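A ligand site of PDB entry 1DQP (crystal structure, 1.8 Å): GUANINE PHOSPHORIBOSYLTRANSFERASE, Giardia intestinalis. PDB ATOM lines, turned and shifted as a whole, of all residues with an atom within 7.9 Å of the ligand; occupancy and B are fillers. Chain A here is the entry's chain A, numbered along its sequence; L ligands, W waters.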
ATOM      1  N   ASP A 125     -13.160  17.485  -9.083  1.00  0.00           N
ATOM      2  CA  ASP A 125     -13.436  16.126  -9.484  1.00  0.00           C
ATOM      3  C   ASP A 125     -14.739  15.779  -8.779  1.00  0.00           C
ATOM      4  O   ASP A 125     -14.951  16.203  -7.654  1.00  0.00           O
ATOM      5  CB  ASP A 125     -12.295  15.218  -9.076  1.00  0.00           C
ATOM      6  CG  ASP A 125     -12.286  13.953  -9.867  1.00  0.00           C
ATOM      7  OD1 ASP A 125     -11.245  13.264  -9.917  1.00  0.00           O
ATOM      8  OD2 ASP A 125     -13.367  13.665 -10.453  1.00  0.00           O
ATOM      9  N   GLU A 126     -15.650  15.082  -9.439  1.00  0.00           N
ATOM     10  CA  GLU A 126     -16.911  14.781  -8.771  1.00  0.00           C
ATOM     11  C   GLU A 126     -16.759  13.717  -7.685  1.00  0.00           C
ATOM     12  O   GLU A 126     -17.554  13.708  -6.722  1.00  0.00           O
ATOM     13  CB  GLU A 126     -17.985  14.350  -9.792  1.00  0.00           C
ATOM     14  CG  GLU A 126     -17.799  12.955 -10.400  1.00  0.00           C
ATOM     15  CD  GLU A 126     -16.709  12.878 -11.463  1.00  0.00           C
ATOM     16  OE1 GLU A 126     -16.719  11.912 -12.251  1.00  0.00           O
ATOM     17  OE2 GLU A 126     -15.839  13.763 -11.508  1.00  0.00           O
ATOM     18  N   TYR A 127     -15.746  12.853  -7.828  1.00  0.00           N
ATOM     19  CA  TYR A 127     -15.505  11.784  -6.850  1.00  0.00           C
ATOM     20  C   TYR A 127     -14.060  11.445  -6.436  1.00  0.00           C
ATOM     21  O   TYR A 127     -13.261  10.953  -7.236  1.00  0.00           O
ATOM     22  CB  TYR A 127     -16.178  10.492  -7.344  1.00  0.00           C
ATOM     23  CG  TYR A 127     -16.254   9.390  -6.305  1.00  0.00           C
ATOM     24  CD1 TYR A 127     -16.407   9.689  -4.954  1.00  0.00           C
ATOM     25  CD2 TYR A 127     -16.247   8.040  -6.686  1.00  0.00           C
ATOM     26  CE1 TYR A 127     -16.544   8.669  -4.004  1.00  0.00           C
ATOM     27  CE2 TYR A 127     -16.393   7.024  -5.736  1.00  0.00           C
ATOM     28  CZ  TYR A 127     -16.540   7.350  -4.396  1.00  0.00           C
ATOM     29  OH  TYR A 127     -16.711   6.348  -3.471  1.00  0.00           O
ATOM     30  N   VAL A 128     -13.747  11.691  -5.165  1.00  0.00           N
ATOM     31  CA  VAL A 128     -12.442  11.354  -4.605  1.00  0.00           C
ATOM     32  C   VAL A 128     -12.665  10.019  -3.902  1.00  0.00           C
ATOM     33  O   VAL A 128     -13.257   9.975  -2.824  1.00  0.00           O
ATOM     34  CB  VAL A 128     -11.970  12.417  -3.601  1.00  0.00           C
ATOM     35  CG1 VAL A 128     -10.738  11.923  -2.854  1.00  0.00           C
ATOM     36  CG2 VAL A 128     -11.649  13.697  -4.328  1.00  0.00           C
ATOM     37  N   ASP A 129     -12.192   8.947  -4.520  1.00  0.00           N
ATOM     38  CA  ASP A 129     -12.370   7.582  -4.024  1.00  0.00           C
ATOM     39  C   ASP A 129     -11.148   7.052  -3.270  1.00  0.00           C
ATOM     40  O   ASP A 129     -11.108   7.070  -2.040  1.00  0.00           O
ATOM     41  CB  ASP A 129     -12.685   6.657  -5.218  1.00  0.00           C
ATOM     42  CG  ASP A 129     -13.166   5.283  -4.792  1.00  0.00           C
ATOM     43  OD1 ASP A 129     -13.161   4.965  -3.582  1.00  0.00           O
ATOM     44  OD2 ASP A 129     -13.548   4.499  -5.702  1.00  0.00           O
ATOM     45  N   SER A 130     -10.168   6.559  -4.017  1.00  0.00           N
ATOM     46  CA  SER A 130      -8.950   6.019  -3.433  1.00  0.00           C
ATOM     47  C   SER A 130      -8.052   7.126  -2.895  1.00  0.00           C
ATOM     48  O   SER A 130      -7.288   6.930  -1.958  1.00  0.00           O
ATOM     49  CB  SER A 130      -8.178   5.215  -4.474  1.00  0.00           C
ATOM     50  OG  SER A 130      -7.778   6.032  -5.552  1.00  0.00           O
ATOM     51  N   THR A 133      -5.108   9.672  -6.365  1.00  0.00           N
ATOM     52  CA  THR A 133      -5.067  10.788  -7.299  1.00  0.00           C
ATOM     53  C   THR A 133      -4.649  12.089  -6.624  1.00  0.00           C
ATOM     54  O   THR A 133      -3.762  12.784  -7.118  1.00  0.00           O
ATOM     55  CB  THR A 133      -6.439  10.998  -7.980  1.00  0.00           C
ATOM     56  OG1 THR A 133      -6.780   9.850  -8.766  1.00  0.00           O
ATOM     57  CG2 THR A 133      -6.414  12.230  -8.877  1.00  0.00           C
ATOM     58  N   LYS A 152     -14.949   9.583  -0.531  1.00  0.00           N
ATOM     59  CA  LYS A 152     -15.163   8.321   0.167  1.00  0.00           C
ATOM     60  C   LYS A 152     -14.741   8.327   1.638  1.00  0.00           C
ATOM     61  O   LYS A 152     -15.497   7.862   2.494  1.00  0.00           O
ATOM     62  CB  LYS A 152     -14.453   7.181  -0.571  1.00  0.00           C
ATOM     63  CG  LYS A 152     -14.467   5.875   0.215  1.00  0.00           C
ATOM     64  CD  LYS A 152     -14.050   4.697  -0.645  1.00  0.00           C
ATOM     65  CE  LYS A 152     -15.255   4.121  -1.392  1.00  0.00           C
ATOM     66  NZ  LYS A 152     -14.848   2.985  -2.251  1.00  0.00           N
ATOM     67  N   GLY A 178     -17.171  -0.756  -0.986  1.00  0.00           N
ATOM     68  CA  GLY A 178     -17.788  -1.768  -1.837  1.00  0.00           C
ATOM     69  C   GLY A 178     -18.787  -1.252  -2.850  1.00  0.00           C
ATOM     70  O   GLY A 178     -19.410  -2.041  -3.568  1.00  0.00           O
ATOM     71  N   SER A 179     -18.970   0.055  -2.922  1.00  0.00           N
ATOM     72  CA  SER A 179     -19.910   0.579  -3.893  1.00  0.00           C
ATOM     73  C   SER A 179     -19.220   0.829  -5.231  1.00  0.00           C
ATOM     74  O   SER A 179     -17.998   0.892  -5.301  1.00  0.00           O
ATOM     75  CB  SER A 179     -20.498   1.893  -3.376  1.00  0.00           C
ATOM     76  OG  SER A 179     -19.491   2.882  -3.190  1.00  0.00           O
ATOM     77  N   TRP A 180     -20.006   0.913  -6.292  1.00  0.00           N
ATOM     78  CA  TRP A 180     -19.486   1.255  -7.603  1.00  0.00           C
ATOM     79  C   TRP A 180     -20.533   2.206  -8.144  1.00  0.00           C
ATOM     80  O   TRP A 180     -21.667   1.817  -8.385  1.00  0.00           O
ATOM     81  CB  TRP A 180     -19.339   0.064  -8.536  1.00  0.00           C
ATOM     82  CG  TRP A 180     -18.713   0.527  -9.828  1.00  0.00           C
ATOM     83  CD1 TRP A 180     -19.358   0.713 -11.020  1.00  0.00           C
ATOM     84  CD2 TRP A 180     -17.372   0.967 -10.027  1.00  0.00           C
ATOM     85  NE1 TRP A 180     -18.496   1.248 -11.953  1.00  0.00           N
ATOM     86  CE2 TRP A 180     -17.265   1.415 -11.366  1.00  0.00           C
ATOM     87  CE3 TRP A 180     -16.237   1.025  -9.198  1.00  0.00           C
ATOM     88  CZ2 TRP A 180     -16.074   1.910 -11.897  1.00  0.00           C
ATOM     89  CZ3 TRP A 180     -15.040   1.531  -9.734  1.00  0.00           C
ATOM     90  CH2 TRP A 180     -14.974   1.968 -11.079  1.00  0.00           C
ATOM     91  N   LEU A 181     -20.125   3.452  -8.318  1.00  0.00           N
ATOM     92  CA  LEU A 181     -21.027   4.502  -8.748  1.00  0.00           C
ATOM     93  C   LEU A 181     -21.121   4.768 -10.245  1.00  0.00           C
ATOM     94  O   LEU A 181     -20.122   4.723 -10.959  1.00  0.00           O
ATOM     95  CB  LEU A 181     -20.632   5.807  -8.056  1.00  0.00           C
ATOM     96  CG  LEU A 181     -20.329   5.813  -6.554  1.00  0.00           C
ATOM     97  CD1 LEU A 181     -19.839   7.202  -6.124  1.00  0.00           C
ATOM     98  CD2 LEU A 181     -21.561   5.400  -5.775  1.00  0.00           C
ATOM     99  N   ILE A 182     -22.332   5.042 -10.713  1.00  0.00           N
ATOM    100  CA  ILE A 182     -22.539   5.406 -12.109  1.00  0.00           C
ATOM    101  C   ILE A 182     -23.594   6.499 -12.073  1.00  0.00           C
ATOM    102  O   ILE A 182     -24.393   6.537 -11.148  1.00  0.00           O
ATOM    103  CB  ILE A 182     -23.008   4.225 -13.010  1.00  0.00           C
ATOM    104  CG1 ILE A 182     -24.428   3.792 -12.645  1.00  0.00           C
ATOM    105  CG2 ILE A 182     -22.020   3.057 -12.905  1.00  0.00           C
ATOM    106  CD1 ILE A 182     -25.510   4.528 -13.461  1.00  0.00           C
ATOM    107  N   GLY A 183     -23.579   7.389 -13.051  1.00  0.00           N
ATOM    108  CA  GLY A 183     -24.550   8.463 -13.041  1.00  0.00           C
ATOM    109  C   GLY A 183     -23.900   9.709 -12.460  1.00  0.00           C
ATOM    110  O   GLY A 183     -22.738   9.661 -12.037  1.00  0.00           O
ATOM    111  N   GLY A 185     -22.735  12.092 -13.911  1.00  0.00           N
ATOM    112  CA  GLY A 185     -21.558  12.348 -14.741  1.00  0.00           C
ATOM    113  C   GLY A 185     -20.577  11.182 -14.825  1.00  0.00           C
ATOM    114  O   GLY A 185     -19.741  11.148 -15.748  1.00  0.00           O
ATOM    115  N   LEU A 186     -20.660  10.253 -13.870  1.00  0.00           N
ATOM    116  CA  LEU A 186     -19.783   9.086 -13.841  1.00  0.00           C
ATOM    117  C   LEU A 186     -20.324   8.080 -14.855  1.00  0.00           C
ATOM    118  O   LEU A 186     -21.526   7.874 -14.941  1.00  0.00           O
ATOM    119  CB  LEU A 186     -19.761   8.474 -12.422  1.00  0.00           C
ATOM    120  CG  LEU A 186     -19.117   9.294 -11.302  1.00  0.00           C
ATOM    121  CD1 LEU A 186     -19.528   8.751  -9.942  1.00  0.00           C
ATOM    122  CD2 LEU A 186     -17.603   9.251 -11.434  1.00  0.00           C
ATOM    123  N   ASP A 187     -19.433   7.456 -15.620  1.00  0.00           N
ATOM    124  CA  ASP A 187     -19.866   6.529 -16.662  1.00  0.00           C
ATOM    125  C   ASP A 187     -20.026   5.088 -16.232  1.00  0.00           C
ATOM    126  O   ASP A 187     -19.405   4.635 -15.275  1.00  0.00           O
ATOM    127  CB  ASP A 187     -18.879   6.520 -17.819  1.00  0.00           C
ATOM    128  CG  ASP A 187     -17.570   5.871 -17.434  1.00  0.00           C
ATOM    129  OD1 ASP A 187     -16.931   6.367 -16.485  1.00  0.00           O
ATOM    130  OD2 ASP A 187     -17.172   4.850 -18.045  1.00  0.00           O
ATOM    131  N   ASP A 188     -20.874   4.387 -16.974  1.00  0.00           N
ATOM    132  CA  ASP A 188     -21.110   2.967 -16.746  1.00  0.00           C
ATOM    133  C   ASP A 188     -20.505   2.379 -18.024  1.00  0.00           C
ATOM    134  O   ASP A 188     -21.176   2.248 -19.061  1.00  0.00           O
ATOM    135  CB  ASP A 188     -22.597   2.678 -16.659  1.00  0.00           C
ATOM    136  CG  ASP A 188     -22.907   1.200 -16.506  1.00  0.00           C
ATOM    137  OD1 ASP A 188     -21.954   0.425 -16.249  1.00  0.00           O
ATOM    138  OD2 ASP A 188     -24.083   0.815 -16.637  1.00  0.00           O
ATOM    139  N   ASN A 189     -19.212   2.091 -17.955  1.00  0.00           N
ATOM    140  CA  ASN A 189     -18.484   1.569 -19.106  1.00  0.00           C
ATOM    141  C   ASN A 189     -18.719   2.502 -20.286  1.00  0.00           C
ATOM    142  O   ASN A 189     -19.066   2.064 -21.393  1.00  0.00           O
ATOM    143  CB  ASN A 189     -18.967   0.151 -19.414  1.00  0.00           C
ATOM    144  CG  ASN A 189     -18.470  -0.851 -18.380  1.00  0.00           C
ATOM    145  OD1 ASN A 189     -19.106  -1.884 -18.131  1.00  0.00           O
ATOM    146  ND2 ASN A 189     -17.312  -0.572 -17.786  1.00  0.00           N
ATOM    147  N   GLY A 190     -18.563   3.797 -20.020  1.00  0.00           N
ATOM    148  CA  GLY A 190     -18.724   4.795 -21.066  1.00  0.00           C
ATOM    149  C   GLY A 190     -20.103   5.396 -21.235  1.00  0.00           C
ATOM    150  O   GLY A 190     -20.240   6.528 -21.720  1.00  0.00           O
ATOM    151  N   LEU A 191     -21.124   4.658 -20.829  1.00  0.00           N
ATOM    152  CA  LEU A 191     -22.505   5.099 -21.001  1.00  0.00           C
ATOM    153  C   LEU A 191     -23.120   5.723 -19.758  1.00  0.00           C
ATOM    154  O   LEU A 191     -22.520   5.778 -18.691  1.00  0.00           O
ATOM    155  CB  LEU A 191     -23.356   3.891 -21.418  1.00  0.00           C
ATOM    156  CG  LEU A 191     -22.792   3.056 -22.564  1.00  0.00           C
ATOM    157  CD1 LEU A 191     -23.673   1.821 -22.801  1.00  0.00           C
ATOM    158  CD2 LEU A 191     -22.709   3.904 -23.823  1.00  0.00           C
ATOM    159  N   ARG A 193     -23.649   8.681 -18.527  1.00  0.00           N
ATOM    160  CA  ARG A 193     -23.111   9.789 -17.730  1.00  0.00           C
ATOM    161  C   ARG A 193     -24.217  10.781 -17.371  1.00  0.00           C
ATOM    162  O   ARG A 193     -24.186  11.371 -16.292  1.00  0.00           O
ATOM    163  CB  ARG A 193     -22.008  10.537 -18.484  1.00  0.00           C
ATOM    164  CG  ARG A 193     -20.665   9.807 -18.537  1.00  0.00           C
ATOM    165  CD  ARG A 193     -19.640  10.707 -19.236  1.00  0.00           C
ATOM    166  NE  ARG A 193     -18.357  10.027 -19.465  1.00  0.00           N
ATOM    167  CZ  ARG A 193     -17.465   9.734 -18.525  1.00  0.00           C
ATOM    168  NH1 ARG A 193     -17.679  10.056 -17.250  1.00  0.00           N
ATOM    169  NH2 ARG A 193     -16.349   9.113 -18.860  1.00  0.00           N
ATOM    170  N   LEU A 198     -27.335   9.831  -8.645  1.00  0.00           N
ATOM    171  CA  LEU A 198     -26.136   9.061  -8.369  1.00  0.00           C
ATOM    172  C   LEU A 198     -26.601   7.641  -8.043  1.00  0.00           C
ATOM    173  O   LEU A 198     -27.326   7.438  -7.072  1.00  0.00           O
ATOM    174  CB  LEU A 198     -25.388   9.617  -7.168  1.00  0.00           C
ATOM    175  CG  LEU A 198     -24.122   8.829  -6.835  1.00  0.00           C
ATOM    176  CD1 LEU A 198     -23.067   9.081  -7.912  1.00  0.00           C
ATOM    177  CD2 LEU A 198     -23.596   9.234  -5.445  1.00  0.00           C
ATOM    178  N   PHE A 199     -26.199   6.677  -8.864  1.00  0.00           N
ATOM    179  CA  PHE A 199     -26.580   5.287  -8.635  1.00  0.00           C
ATOM    180  C   PHE A 199     -25.375   4.467  -8.221  1.00  0.00           C
ATOM    181  O   PHE A 199     -24.230   4.822  -8.507  1.00  0.00           O
ATOM    182  CB  PHE A 199     -27.119   4.639  -9.928  1.00  0.00           C
ATOM    183  CG  PHE A 199     -28.446   5.171 -10.382  1.00  0.00           C
ATOM    184  CD1 PHE A 199     -28.515   6.152 -11.374  1.00  0.00           C
ATOM    185  CD2 PHE A 199     -29.626   4.653  -9.867  1.00  0.00           C
ATOM    186  CE1 PHE A 199     -29.750   6.602 -11.841  1.00  0.00           C
ATOM    187  CE2 PHE A 199     -30.858   5.107 -10.320  1.00  0.00           C
ATOM    188  CZ  PHE A 199     -30.919   6.084 -11.312  1.00  0.00           C
ATOM    189  N   ASP A 200     -25.658   3.360  -7.554  1.00  0.00           N
ATOM    190  CA  ASP A 200     -24.629   2.398  -7.165  1.00  0.00           C
ATOM    191  C   ASP A 200     -25.085   1.080  -7.791  1.00  0.00           C
ATOM    192  O   ASP A 200     -26.287   0.860  -7.970  1.00  0.00           O
ATOM    193  CB  ASP A 200     -24.578   2.200  -5.656  1.00  0.00           C
ATOM    194  CG  ASP A 200     -24.011   0.853  -5.287  1.00  0.00           C
ATOM    195  OD1 ASP A 200     -22.785   0.659  -5.425  1.00  0.00           O
ATOM    196  OD2 ASP A 200     -24.798  -0.042  -4.901  1.00  0.00           O
ATOM    197  N   ILE A 201     -24.137   0.201  -8.102  1.00  0.00           N
ATOM    198  CA  ILE A 201     -24.520  -1.086  -8.674  1.00  0.00           C
ATOM    199  C   ILE A 201     -23.931  -2.264  -7.907  1.00  0.00           C
ATOM    200  O   ILE A 201     -24.129  -3.414  -8.310  1.00  0.00           O
ATOM    201  CB  ILE A 201     -24.100  -1.249 -10.162  1.00  0.00           C
ATOM    202  CG1 ILE A 201     -22.590  -1.108 -10.329  1.00  0.00           C
ATOM    203  CG2 ILE A 201     -24.867  -0.245 -11.032  1.00  0.00           C
ATOM    204  CD1 ILE A 201     -22.111  -1.417 -11.742  1.00  0.00           C
HETATM  205  C1  LIG L   1     -13.702   5.971 -10.544  1.00  0.00           C
HETATM  206  C2  LIG L   1     -13.410   5.719  -9.236  1.00  0.00           C
HETATM  207  N1  LIG L   1     -14.406   5.219  -8.540  1.00  0.00           N
HETATM  208  C3  LIG L   1     -15.442   5.140  -9.457  1.00  0.00           C
HETATM  209  C4  LIG L   1     -16.795   4.675  -9.293  1.00  0.00           C
HETATM  210  O1  LIG L   1     -17.347   4.239  -8.278  1.00  0.00           O
HETATM  211  N2  LIG L   1     -17.523   4.759 -10.491  1.00  0.00           N
HETATM  212  N3  LIG L   1     -17.846   5.240 -12.761  1.00  0.00           N
HETATM  213  C5  LIG L   1     -17.016   5.228 -11.717  1.00  0.00           C
HETATM  214  N4  LIG L   1     -15.741   5.663 -11.859  1.00  0.00           N
HETATM  215  C6  LIG L   1     -15.013   5.593 -10.689  1.00  0.00           C
HETATM  216  O   HOH W   1     -16.082   3.059  -6.223  1.00  0.00           O
HETATM  217  O   HOH W   2     -10.349   6.065  -7.585  1.00  0.00           O
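A nitrogen (N2) of the ligand lies within hydrogen-bond range of the backbone carbonyl oxygen of Leu 181, 2.6 Å away. The side-chain carboxylate (OD2) of Asp 129 is in hydrogen-bond range of a nitrogen (N1) of the ligand (3.1 Å). A nitrogen (N3) of the ligand is in hydrogen-bond range of the backbone carbonyl oxygen (O) of Asp 187 (3.0 Å). The backbone NH (N) of Leu 181 sits at hydrogen-bond distance from an oxygen (O1) of the ligand, 2.9 Å away.
The side-chain carboxylate (OD1) of Asp 129 lies within salt-bridge range of the side-chain amino group (NZ) of Lys 152 (2.9 Å). N of Trp 180 is in hydrogen-bond range of OD1 of Asp 200. OD1 of Asp 187 lies within salt-bridge range of NH2 of Arg 193. N of Gly 190 sits at hydrogen-bond distance from OD2 of Asp 187 (2.6 Å). OD2 of Asp 187 sits at hydrogen-bond distance from N of Asn 189 (3.4 Å). O of Trp 180 lies within hydrogen-bond range of N of Ile 201, at 3.0 Å.
Merely in contact with the ligand: Trp 180 (3.5 Å), Leu 186 (3.8 Å) and Tyr 127 (3.8 Å). Hydrophobic or aromatic side chains within 4 Å of the ligand: Tyr 127, Trp 180, Leu 181 and Leu 186. Of the 26 residues printed, 6 come within 4 Å of the ligand. The nearest printed residue that does not touch the ligand is Ser 179 (4.5 Å).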
